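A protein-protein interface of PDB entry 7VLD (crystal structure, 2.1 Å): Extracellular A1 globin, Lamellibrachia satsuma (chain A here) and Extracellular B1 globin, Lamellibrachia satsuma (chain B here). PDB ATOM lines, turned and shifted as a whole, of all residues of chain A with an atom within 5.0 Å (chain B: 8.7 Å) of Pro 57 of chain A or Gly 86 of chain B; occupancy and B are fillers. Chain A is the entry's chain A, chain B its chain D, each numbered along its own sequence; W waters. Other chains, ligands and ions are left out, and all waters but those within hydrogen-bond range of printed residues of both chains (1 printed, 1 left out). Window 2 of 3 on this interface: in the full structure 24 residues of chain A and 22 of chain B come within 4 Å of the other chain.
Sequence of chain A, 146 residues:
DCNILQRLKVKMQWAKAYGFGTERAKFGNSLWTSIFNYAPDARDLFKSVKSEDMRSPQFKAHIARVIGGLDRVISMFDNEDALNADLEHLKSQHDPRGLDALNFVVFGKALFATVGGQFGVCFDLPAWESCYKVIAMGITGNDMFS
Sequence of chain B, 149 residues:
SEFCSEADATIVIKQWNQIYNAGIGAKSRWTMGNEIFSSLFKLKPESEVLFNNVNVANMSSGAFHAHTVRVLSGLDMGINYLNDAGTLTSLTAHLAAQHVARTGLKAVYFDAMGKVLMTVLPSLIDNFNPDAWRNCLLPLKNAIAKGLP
Hydrophobic or aromatic side chains of chain B within 4 Å of the printed part of chain A: Leu 91.
Along chain A the printed residues that touch a printed residue of chain B span positions 57 to 61.
Among the printed residues, 8 pairs touch across the chains.
Of chain B, only Gly 86, Thr 87 and Ser 90 come within 4 Å of Pro 57 of chain A.
Gly 86 of chain B touches one residue of chain A.
Ser 56 of chain A touches none of the printed residues of chain B.
Of the printed residues of chain A, Ser 90 of chain B touches Pro 57, Gln 58 and Ala 61.
Of the printed residues of chain A, Leu 91 of chain B touches Ala 61.
Printed residues of chain A within 4 Å of Thr 87 of chain B: Pro 57 (3.9 Å), Lys 60 (3.3 Å) and Ala 61 (3.7 Å).
Thr 92 of chain B touches none of the printed residues of chain A.
The nearest residue of chain B that does not touch Pro 57 of chain A is Leu 91 of chain B (5.7 Å).
The nearest printed residue of chain A that does not touch Gly 86 of chain B is Gln 58 of chain A (6.1 Å).
The nearest printed residue of chain B that does not touch Ala 61 of chain A is Tyr 81 of chain B (6.2 Å).
O of Arg 55 of chain A lies close to NZ of Lys 60 of chain A, 3.3 Å away.
OD2 of Asp 84 of chain B lies within hydrogen-bond range of OG1 of Thr 87 of chain B, 3.0 Å away.
Water W1 bridges OH of Tyr 81 of chain B (2.7 Å) and O of Lys 60 of chain A (2.9 Å).
Gly 86 of chain B touches Pro 57 of chain A (O to CB, 3.3 Å).
Pro 57 of chain A touches Thr 87 of chain B (CB to N, 3.9 Å).
Pro 57 of chain A touches Ser 90 of chain B.
Gln 58 of chain A touches Ser 90 of chain B (CA to OG, 3.8 Å).
CD of Lys 60 of chain A touches OG1 of Thr 87 of chain B, at 3.3 Å.
Ala 61 of chain A touches Thr 87 of chain B (N to CG2, 3.7 Å).
Ala 61 of chain A touches Ser 90 of chain B (CB to OG, 3.6 Å).
CD2 of Leu 91 of chain B touches O of Ala 61 of chain A (3.5 Å).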
ATOM      1  N   ARG A  55      12.542 -18.139 -38.226  1.00  0.00           N
ATOM      2  CA  ARG A  55      11.270 -17.784 -37.612  1.00  0.00           C
ATOM      3  C   ARG A  55      11.199 -18.176 -36.141  1.00  0.00           C
ATOM      4  O   ARG A  55      10.183 -17.913 -35.494  1.00  0.00           O
ATOM      5  CB  ARG A  55      10.102 -18.418 -38.383  1.00  0.00           C
ATOM      6  CG  ARG A  55      10.133 -19.932 -38.492  1.00  0.00           C
ATOM      7  CD  ARG A  55      10.208 -20.365 -39.951  1.00  0.00           C
ATOM      8  NE  ARG A  55       9.871 -21.775 -40.131  1.00  0.00           N
ATOM      9  CZ  ARG A  55       8.780 -22.212 -40.752  1.00  0.00           C
ATOM     10  NH1 ARG A  55       8.557 -23.514 -40.864  1.00  0.00           N
ATOM     11  NH2 ARG A  55       7.918 -21.349 -41.269  1.00  0.00           N
ATOM     12  N   SER A  56      12.251 -18.789 -35.602  1.00  0.00           N
ATOM     13  CA  SER A  56      12.294 -19.084 -34.180  1.00  0.00           C
ATOM     14  C   SER A  56      12.245 -17.783 -33.380  1.00  0.00           C
ATOM     15  O   SER A  56      12.683 -16.734 -33.862  1.00  0.00           O
ATOM     16  CB  SER A  56      13.563 -19.857 -33.833  1.00  0.00           C
ATOM     17  OG  SER A  56      14.702 -19.015 -33.911  1.00  0.00           O
ATOM     18  N   PRO A  57      11.710 -17.821 -32.159  1.00  0.00           N
ATOM     19  CA  PRO A  57      11.700 -16.599 -31.339  1.00  0.00           C
ATOM     20  C   PRO A  57      13.092 -16.076 -31.033  1.00  0.00           C
ATOM     21  O   PRO A  57      13.258 -14.868 -30.820  1.00  0.00           O
ATOM     22  CB  PRO A  57      10.965 -17.038 -30.064  1.00  0.00           C
ATOM     23  CG  PRO A  57      11.119 -18.525 -30.025  1.00  0.00           C
ATOM     24  CD  PRO A  57      11.102 -18.964 -31.457  1.00  0.00           C
ATOM     25  N   GLN A  58      14.102 -16.949 -31.021  1.00  0.00           N
ATOM     26  CA  GLN A  58      15.456 -16.514 -30.693  1.00  0.00           C
ATOM     27  C   GLN A  58      16.035 -15.623 -31.783  1.00  0.00           C
ATOM     28  O   GLN A  58      16.644 -14.588 -31.486  1.00  0.00           O
ATOM     29  CB  GLN A  58      16.360 -17.727 -30.459  1.00  0.00           C
ATOM     30  CG  GLN A  58      16.089 -18.472 -29.159  1.00  0.00           C
ATOM     31  CD  GLN A  58      14.766 -19.210 -29.173  1.00  0.00           C
ATOM     32  OE1 GLN A  58      14.366 -19.770 -30.193  1.00  0.00           O
ATOM     33  NE2 GLN A  58      14.073 -19.202 -28.040  1.00  0.00           N
ATOM     34  N   PHE A  59      15.864 -16.002 -33.051  1.00  0.00           N
ATOM     35  CA  PHE A  59      16.409 -15.179 -34.125  1.00  0.00           C
ATOM     36  C   PHE A  59      15.543 -13.960 -34.404  1.00  0.00           C
ATOM     37  O   PHE A  59      16.073 -12.903 -34.763  1.00  0.00           O
ATOM     38  CB  PHE A  59      16.591 -16.002 -35.402  1.00  0.00           C
ATOM     39  CG  PHE A  59      17.433 -15.315 -36.439  1.00  0.00           C
ATOM     40  CD1 PHE A  59      18.806 -15.216 -36.274  1.00  0.00           C
ATOM     41  CD2 PHE A  59      16.857 -14.755 -37.565  1.00  0.00           C
ATOM     42  CE1 PHE A  59      19.589 -14.576 -37.218  1.00  0.00           C
ATOM     43  CE2 PHE A  59      17.637 -14.114 -38.514  1.00  0.00           C
ATOM     44  CZ  PHE A  59      19.003 -14.025 -38.339  1.00  0.00           C
ATOM     45  N   LYS A  60      14.221 -14.085 -34.254  1.00  0.00           N
ATOM     46  CA  LYS A  60      13.356 -12.912 -34.334  1.00  0.00           C
ATOM     47  C   LYS A  60      13.751 -11.869 -33.296  1.00  0.00           C
ATOM     48  O   LYS A  60      13.711 -10.663 -33.569  1.00  0.00           O
ATOM     49  CB  LYS A  60      11.895 -13.317 -34.140  1.00  0.00           C
ATOM     50  CG  LYS A  60      11.259 -14.031 -35.320  1.00  0.00           C
ATOM     51  CD  LYS A  60       9.853 -14.485 -34.956  1.00  0.00           C
ATOM     52  CE  LYS A  60       9.101 -15.025 -36.158  1.00  0.00           C
ATOM     53  NZ  LYS A  60       7.815 -15.659 -35.752  1.00  0.00           N
ATOM     54  N   ALA A  61      14.132 -12.316 -32.097  1.00  0.00           N
ATOM     55  CA  ALA A  61      14.593 -11.385 -31.072  1.00  0.00           C
ATOM     56  C   ALA A  61      15.887 -10.702 -31.495  1.00  0.00           C
ATOM     57  O   ALA A  61      16.058  -9.496 -31.279  1.00  0.00           O
ATOM     58  CB  ALA A  61      14.780 -12.114 -29.743  1.00  0.00           C
ATOM     59  N   GLU B   2       0.557 -15.475 -23.039  1.00  0.00           N
ATOM     60  CA  GLU B   2       0.860 -14.587 -21.925  1.00  0.00           C
ATOM     61  C   GLU B   2       0.824 -13.109 -22.331  1.00  0.00           C
ATOM     62  O   GLU B   2       0.417 -12.770 -23.445  1.00  0.00           O
ATOM     63  CB  GLU B   2       2.226 -14.945 -21.319  1.00  0.00           C
ATOM     64  CG  GLU B   2       3.346 -15.176 -22.333  1.00  0.00           C
ATOM     65  CD  GLU B   2       4.568 -15.842 -21.714  1.00  0.00           C
ATOM     66  OE1 GLU B   2       4.862 -17.004 -22.069  1.00  0.00           O
ATOM     67  OE2 GLU B   2       5.230 -15.207 -20.866  1.00  0.00           O
ATOM     68  N   PHE B   3       1.227 -12.255 -21.383  1.00  0.00           N
ATOM     69  CA  PHE B   3       1.358 -10.802 -21.514  1.00  0.00           C
ATOM     70  C   PHE B   3       0.011 -10.082 -21.478  1.00  0.00           C
ATOM     71  O   PHE B   3      -0.619 -10.031 -20.417  1.00  0.00           O
ATOM     72  CB  PHE B   3       2.173 -10.449 -22.761  1.00  0.00           C
ATOM     73  CG  PHE B   3       3.648 -10.637 -22.558  1.00  0.00           C
ATOM     74  CD1 PHE B   3       4.356  -9.757 -21.756  1.00  0.00           C
ATOM     75  CD2 PHE B   3       4.316 -11.713 -23.117  1.00  0.00           C
ATOM     76  CE1 PHE B   3       5.707  -9.928 -21.537  1.00  0.00           C
ATOM     77  CE2 PHE B   3       5.672 -11.889 -22.902  1.00  0.00           C
ATOM     78  CZ  PHE B   3       6.367 -10.994 -22.111  1.00  0.00           C
ATOM     79  N   TYR B  81       6.315  -5.680 -29.956  1.00  0.00           N
ATOM     80  CA  TYR B  81       6.219  -7.133 -30.044  1.00  0.00           C
ATOM     81  C   TYR B  81       5.240  -7.704 -29.020  1.00  0.00           C
ATOM     82  O   TYR B  81       5.357  -8.865 -28.622  1.00  0.00           O
ATOM     83  CB  TYR B  81       7.597  -7.773 -29.884  1.00  0.00           C
ATOM     84  CG  TYR B  81       8.434  -7.717 -31.141  1.00  0.00           C
ATOM     85  CD1 TYR B  81       9.174  -6.587 -31.455  1.00  0.00           C
ATOM     86  CD2 TYR B  81       8.475  -8.793 -32.019  1.00  0.00           C
ATOM     87  CE1 TYR B  81       9.937  -6.529 -32.605  1.00  0.00           C
ATOM     88  CE2 TYR B  81       9.235  -8.744 -33.171  1.00  0.00           C
ATOM     89  CZ  TYR B  81       9.964  -7.611 -33.460  1.00  0.00           C
ATOM     90  OH  TYR B  81      10.723  -7.555 -34.606  1.00  0.00           O
ATOM     91  N   LEU B  82       4.260  -6.899 -28.597  1.00  0.00           N
ATOM     92  CA  LEU B  82       3.281  -7.371 -27.624  1.00  0.00           C
ATOM     93  C   LEU B  82       2.390  -8.466 -28.197  1.00  0.00           C
ATOM     94  O   LEU B  82       1.961  -9.361 -27.459  1.00  0.00           O
ATOM     95  CB  LEU B  82       2.430  -6.202 -27.124  1.00  0.00           C
ATOM     96  CG  LEU B  82       3.060  -5.260 -26.094  1.00  0.00           C
ATOM     97  CD1 LEU B  82       2.203  -4.014 -25.911  1.00  0.00           C
ATOM     98  CD2 LEU B  82       3.269  -5.968 -24.765  1.00  0.00           C
ATOM     99  N   ASN B  83       2.096  -8.417 -29.495  1.00  0.00           N
ATOM    100  CA  ASN B  83       1.275  -9.427 -30.149  1.00  0.00           C
ATOM    101  C   ASN B  83       2.089 -10.608 -30.665  1.00  0.00           C
ATOM    102  O   ASN B  83       1.564 -11.419 -31.435  1.00  0.00           O
ATOM    103  CB  ASN B  83       0.480  -8.799 -31.297  1.00  0.00           C
ATOM    104  CG  ASN B  83      -0.663  -7.933 -30.806  1.00  0.00           C
ATOM    105  OD1 ASN B  83      -1.345  -8.276 -29.840  1.00  0.00           O
ATOM    106  ND2 ASN B  83      -0.875  -6.801 -31.467  1.00  0.00           N
ATOM    107  N   ASP B  84       3.356 -10.720 -30.260  1.00  0.00           N
ATOM    108  CA  ASP B  84       4.232 -11.833 -30.630  1.00  0.00           C
ATOM    109  C   ASP B  84       4.806 -12.379 -29.325  1.00  0.00           C
ATOM    110  O   ASP B  84       5.959 -12.111 -28.980  1.00  0.00           O
ATOM    111  CB  ASP B  84       5.324 -11.376 -31.599  1.00  0.00           C
ATOM    112  CG  ASP B  84       6.070 -12.534 -32.235  1.00  0.00           C
ATOM    113  OD1 ASP B  84       6.039 -13.655 -31.684  1.00  0.00           O
ATOM    114  OD2 ASP B  84       6.695 -12.321 -33.295  1.00  0.00           O
ATOM    115  N   ALA B  85       3.987 -13.152 -28.604  1.00  0.00           N
ATOM    116  CA  ALA B  85       4.360 -13.597 -27.264  1.00  0.00           C
ATOM    117  C   ALA B  85       5.641 -14.420 -27.280  1.00  0.00           C
ATOM    118  O   ALA B  85       6.459 -14.324 -26.358  1.00  0.00           O
ATOM    119  CB  ALA B  85       3.218 -14.399 -26.642  1.00  0.00           C
ATOM    120  N   GLY B  86       5.833 -15.238 -28.316  1.00  0.00           N
ATOM    121  CA  GLY B  86       7.042 -16.041 -28.391  1.00  0.00           C
ATOM    122  C   GLY B  86       8.296 -15.192 -28.464  1.00  0.00           C
ATOM    123  O   GLY B  86       9.250 -15.402 -27.708  1.00  0.00           O
ATOM    124  N   THR B  87       8.307 -14.211 -29.368  1.00  0.00           N
ATOM    125  CA  THR B  87       9.478 -13.353 -29.512  1.00  0.00           C
ATOM    126  C   THR B  87       9.645 -12.437 -28.306  1.00  0.00           C
ATOM    127  O   THR B  87      10.769 -12.230 -27.831  1.00  0.00           O
ATOM    128  CB  THR B  87       9.372 -12.533 -30.797  1.00  0.00           C
ATOM    129  OG1 THR B  87       9.180 -13.413 -31.911  1.00  0.00           O
ATOM    130  CG2 THR B  87      10.639 -11.720 -31.013  1.00  0.00           C
ATOM    131  N   LEU B  88       8.542 -11.879 -27.800  1.00  0.00           N
ATOM    132  CA  LEU B  88       8.627 -10.993 -26.644  1.00  0.00           C
ATOM    133  C   LEU B  88       9.192 -11.713 -25.427  1.00  0.00           C
ATOM    134  O   LEU B  88       9.899 -11.103 -24.617  1.00  0.00           O
ATOM    135  CB  LEU B  88       7.250 -10.408 -26.325  1.00  0.00           C
ATOM    136  CG  LEU B  88       7.212  -9.349 -25.223  1.00  0.00           C
ATOM    137  CD1 LEU B  88       8.153  -8.202 -25.552  1.00  0.00           C
ATOM    138  CD2 LEU B  88       5.795  -8.840 -25.009  1.00  0.00           C
ATOM    139  N   THR B  89       8.895 -13.007 -25.285  1.00  0.00           N
ATOM    140  CA  THR B  89       9.484 -13.789 -24.203  1.00  0.00           C
ATOM    141  C   THR B  89      11.002 -13.837 -24.332  1.00  0.00           C
ATOM    142  O   THR B  89      11.729 -13.602 -23.358  1.00  0.00           O
ATOM    143  CB  THR B  89       8.899 -15.202 -24.201  1.00  0.00           C
ATOM    144  OG1 THR B  89       7.476 -15.131 -24.042  1.00  0.00           O
ATOM    145  CG2 THR B  89       9.492 -16.025 -23.068  1.00  0.00           C
ATOM    146  N   SER B  90      11.500 -14.133 -25.534  1.00  0.00           N
ATOM    147  CA  SER B  90      12.943 -14.173 -25.749  1.00  0.00           C
ATOM    148  C   SER B  90      13.561 -12.787 -25.604  1.00  0.00           C
ATOM    149  O   SER B  90      14.676 -12.650 -25.086  1.00  0.00           O
ATOM    150  CB  SER B  90      13.249 -14.761 -27.127  1.00  0.00           C
ATOM    151  OG  SER B  90      14.643 -14.772 -27.380  1.00  0.00           O
ATOM    152  N   LEU B  91      12.851 -11.747 -26.053  1.00  0.00           N
ATOM    153  CA  LEU B  91      13.364 -10.385 -25.928  1.00  0.00           C
ATOM    154  C   LEU B  91      13.489  -9.970 -24.468  1.00  0.00           C
ATOM    155  O   LEU B  91      14.482  -9.345 -24.074  1.00  0.00           O
ATOM    156  CB  LEU B  91      12.457  -9.412 -26.683  1.00  0.00           C
ATOM    157  CG  LEU B  91      12.571  -9.400 -28.208  1.00  0.00           C
ATOM    158  CD1 LEU B  91      11.377  -8.693 -28.832  1.00  0.00           C
ATOM    159  CD2 LEU B  91      13.868  -8.729 -28.627  1.00  0.00           C
ATOM    160  N   THR B  92      12.488 -10.300 -23.648  1.00  0.00           N
ATOM    161  CA  THR B  92      12.546  -9.931 -22.237  1.00  0.00           C
ATOM    162  C   THR B  92      13.532 -10.800 -21.468  1.00  0.00           C
ATOM    163  O   THR B  92      14.142 -10.331 -20.501  1.00  0.00           O
ATOM    164  CB  THR B  92      11.158 -10.018 -21.605  1.00  0.00           C
ATOM    165  OG1 THR B  92      10.606 -11.323 -21.824  1.00  0.00           O
ATOM    166  CG2 THR B  92      10.235  -8.974 -22.207  1.00  0.00           C
ATOM    167  N   ALA B  93      13.696 -12.063 -21.873  1.00  0.00           N
ATOM    168  CA  ALA B  93      14.712 -12.904 -21.251  1.00  0.00           C
ATOM    169  C   ALA B  93      16.106 -12.334 -21.481  1.00  0.00           C
ATOM    170  O   ALA B  93      16.950 -12.349 -20.577  1.00  0.00           O
ATOM    171  CB  ALA B  93      14.617 -14.331 -21.788  1.00  0.00           C
HETATM  172  O   HOH W   1      11.674  -9.931 -35.487  1.00  0.00           O
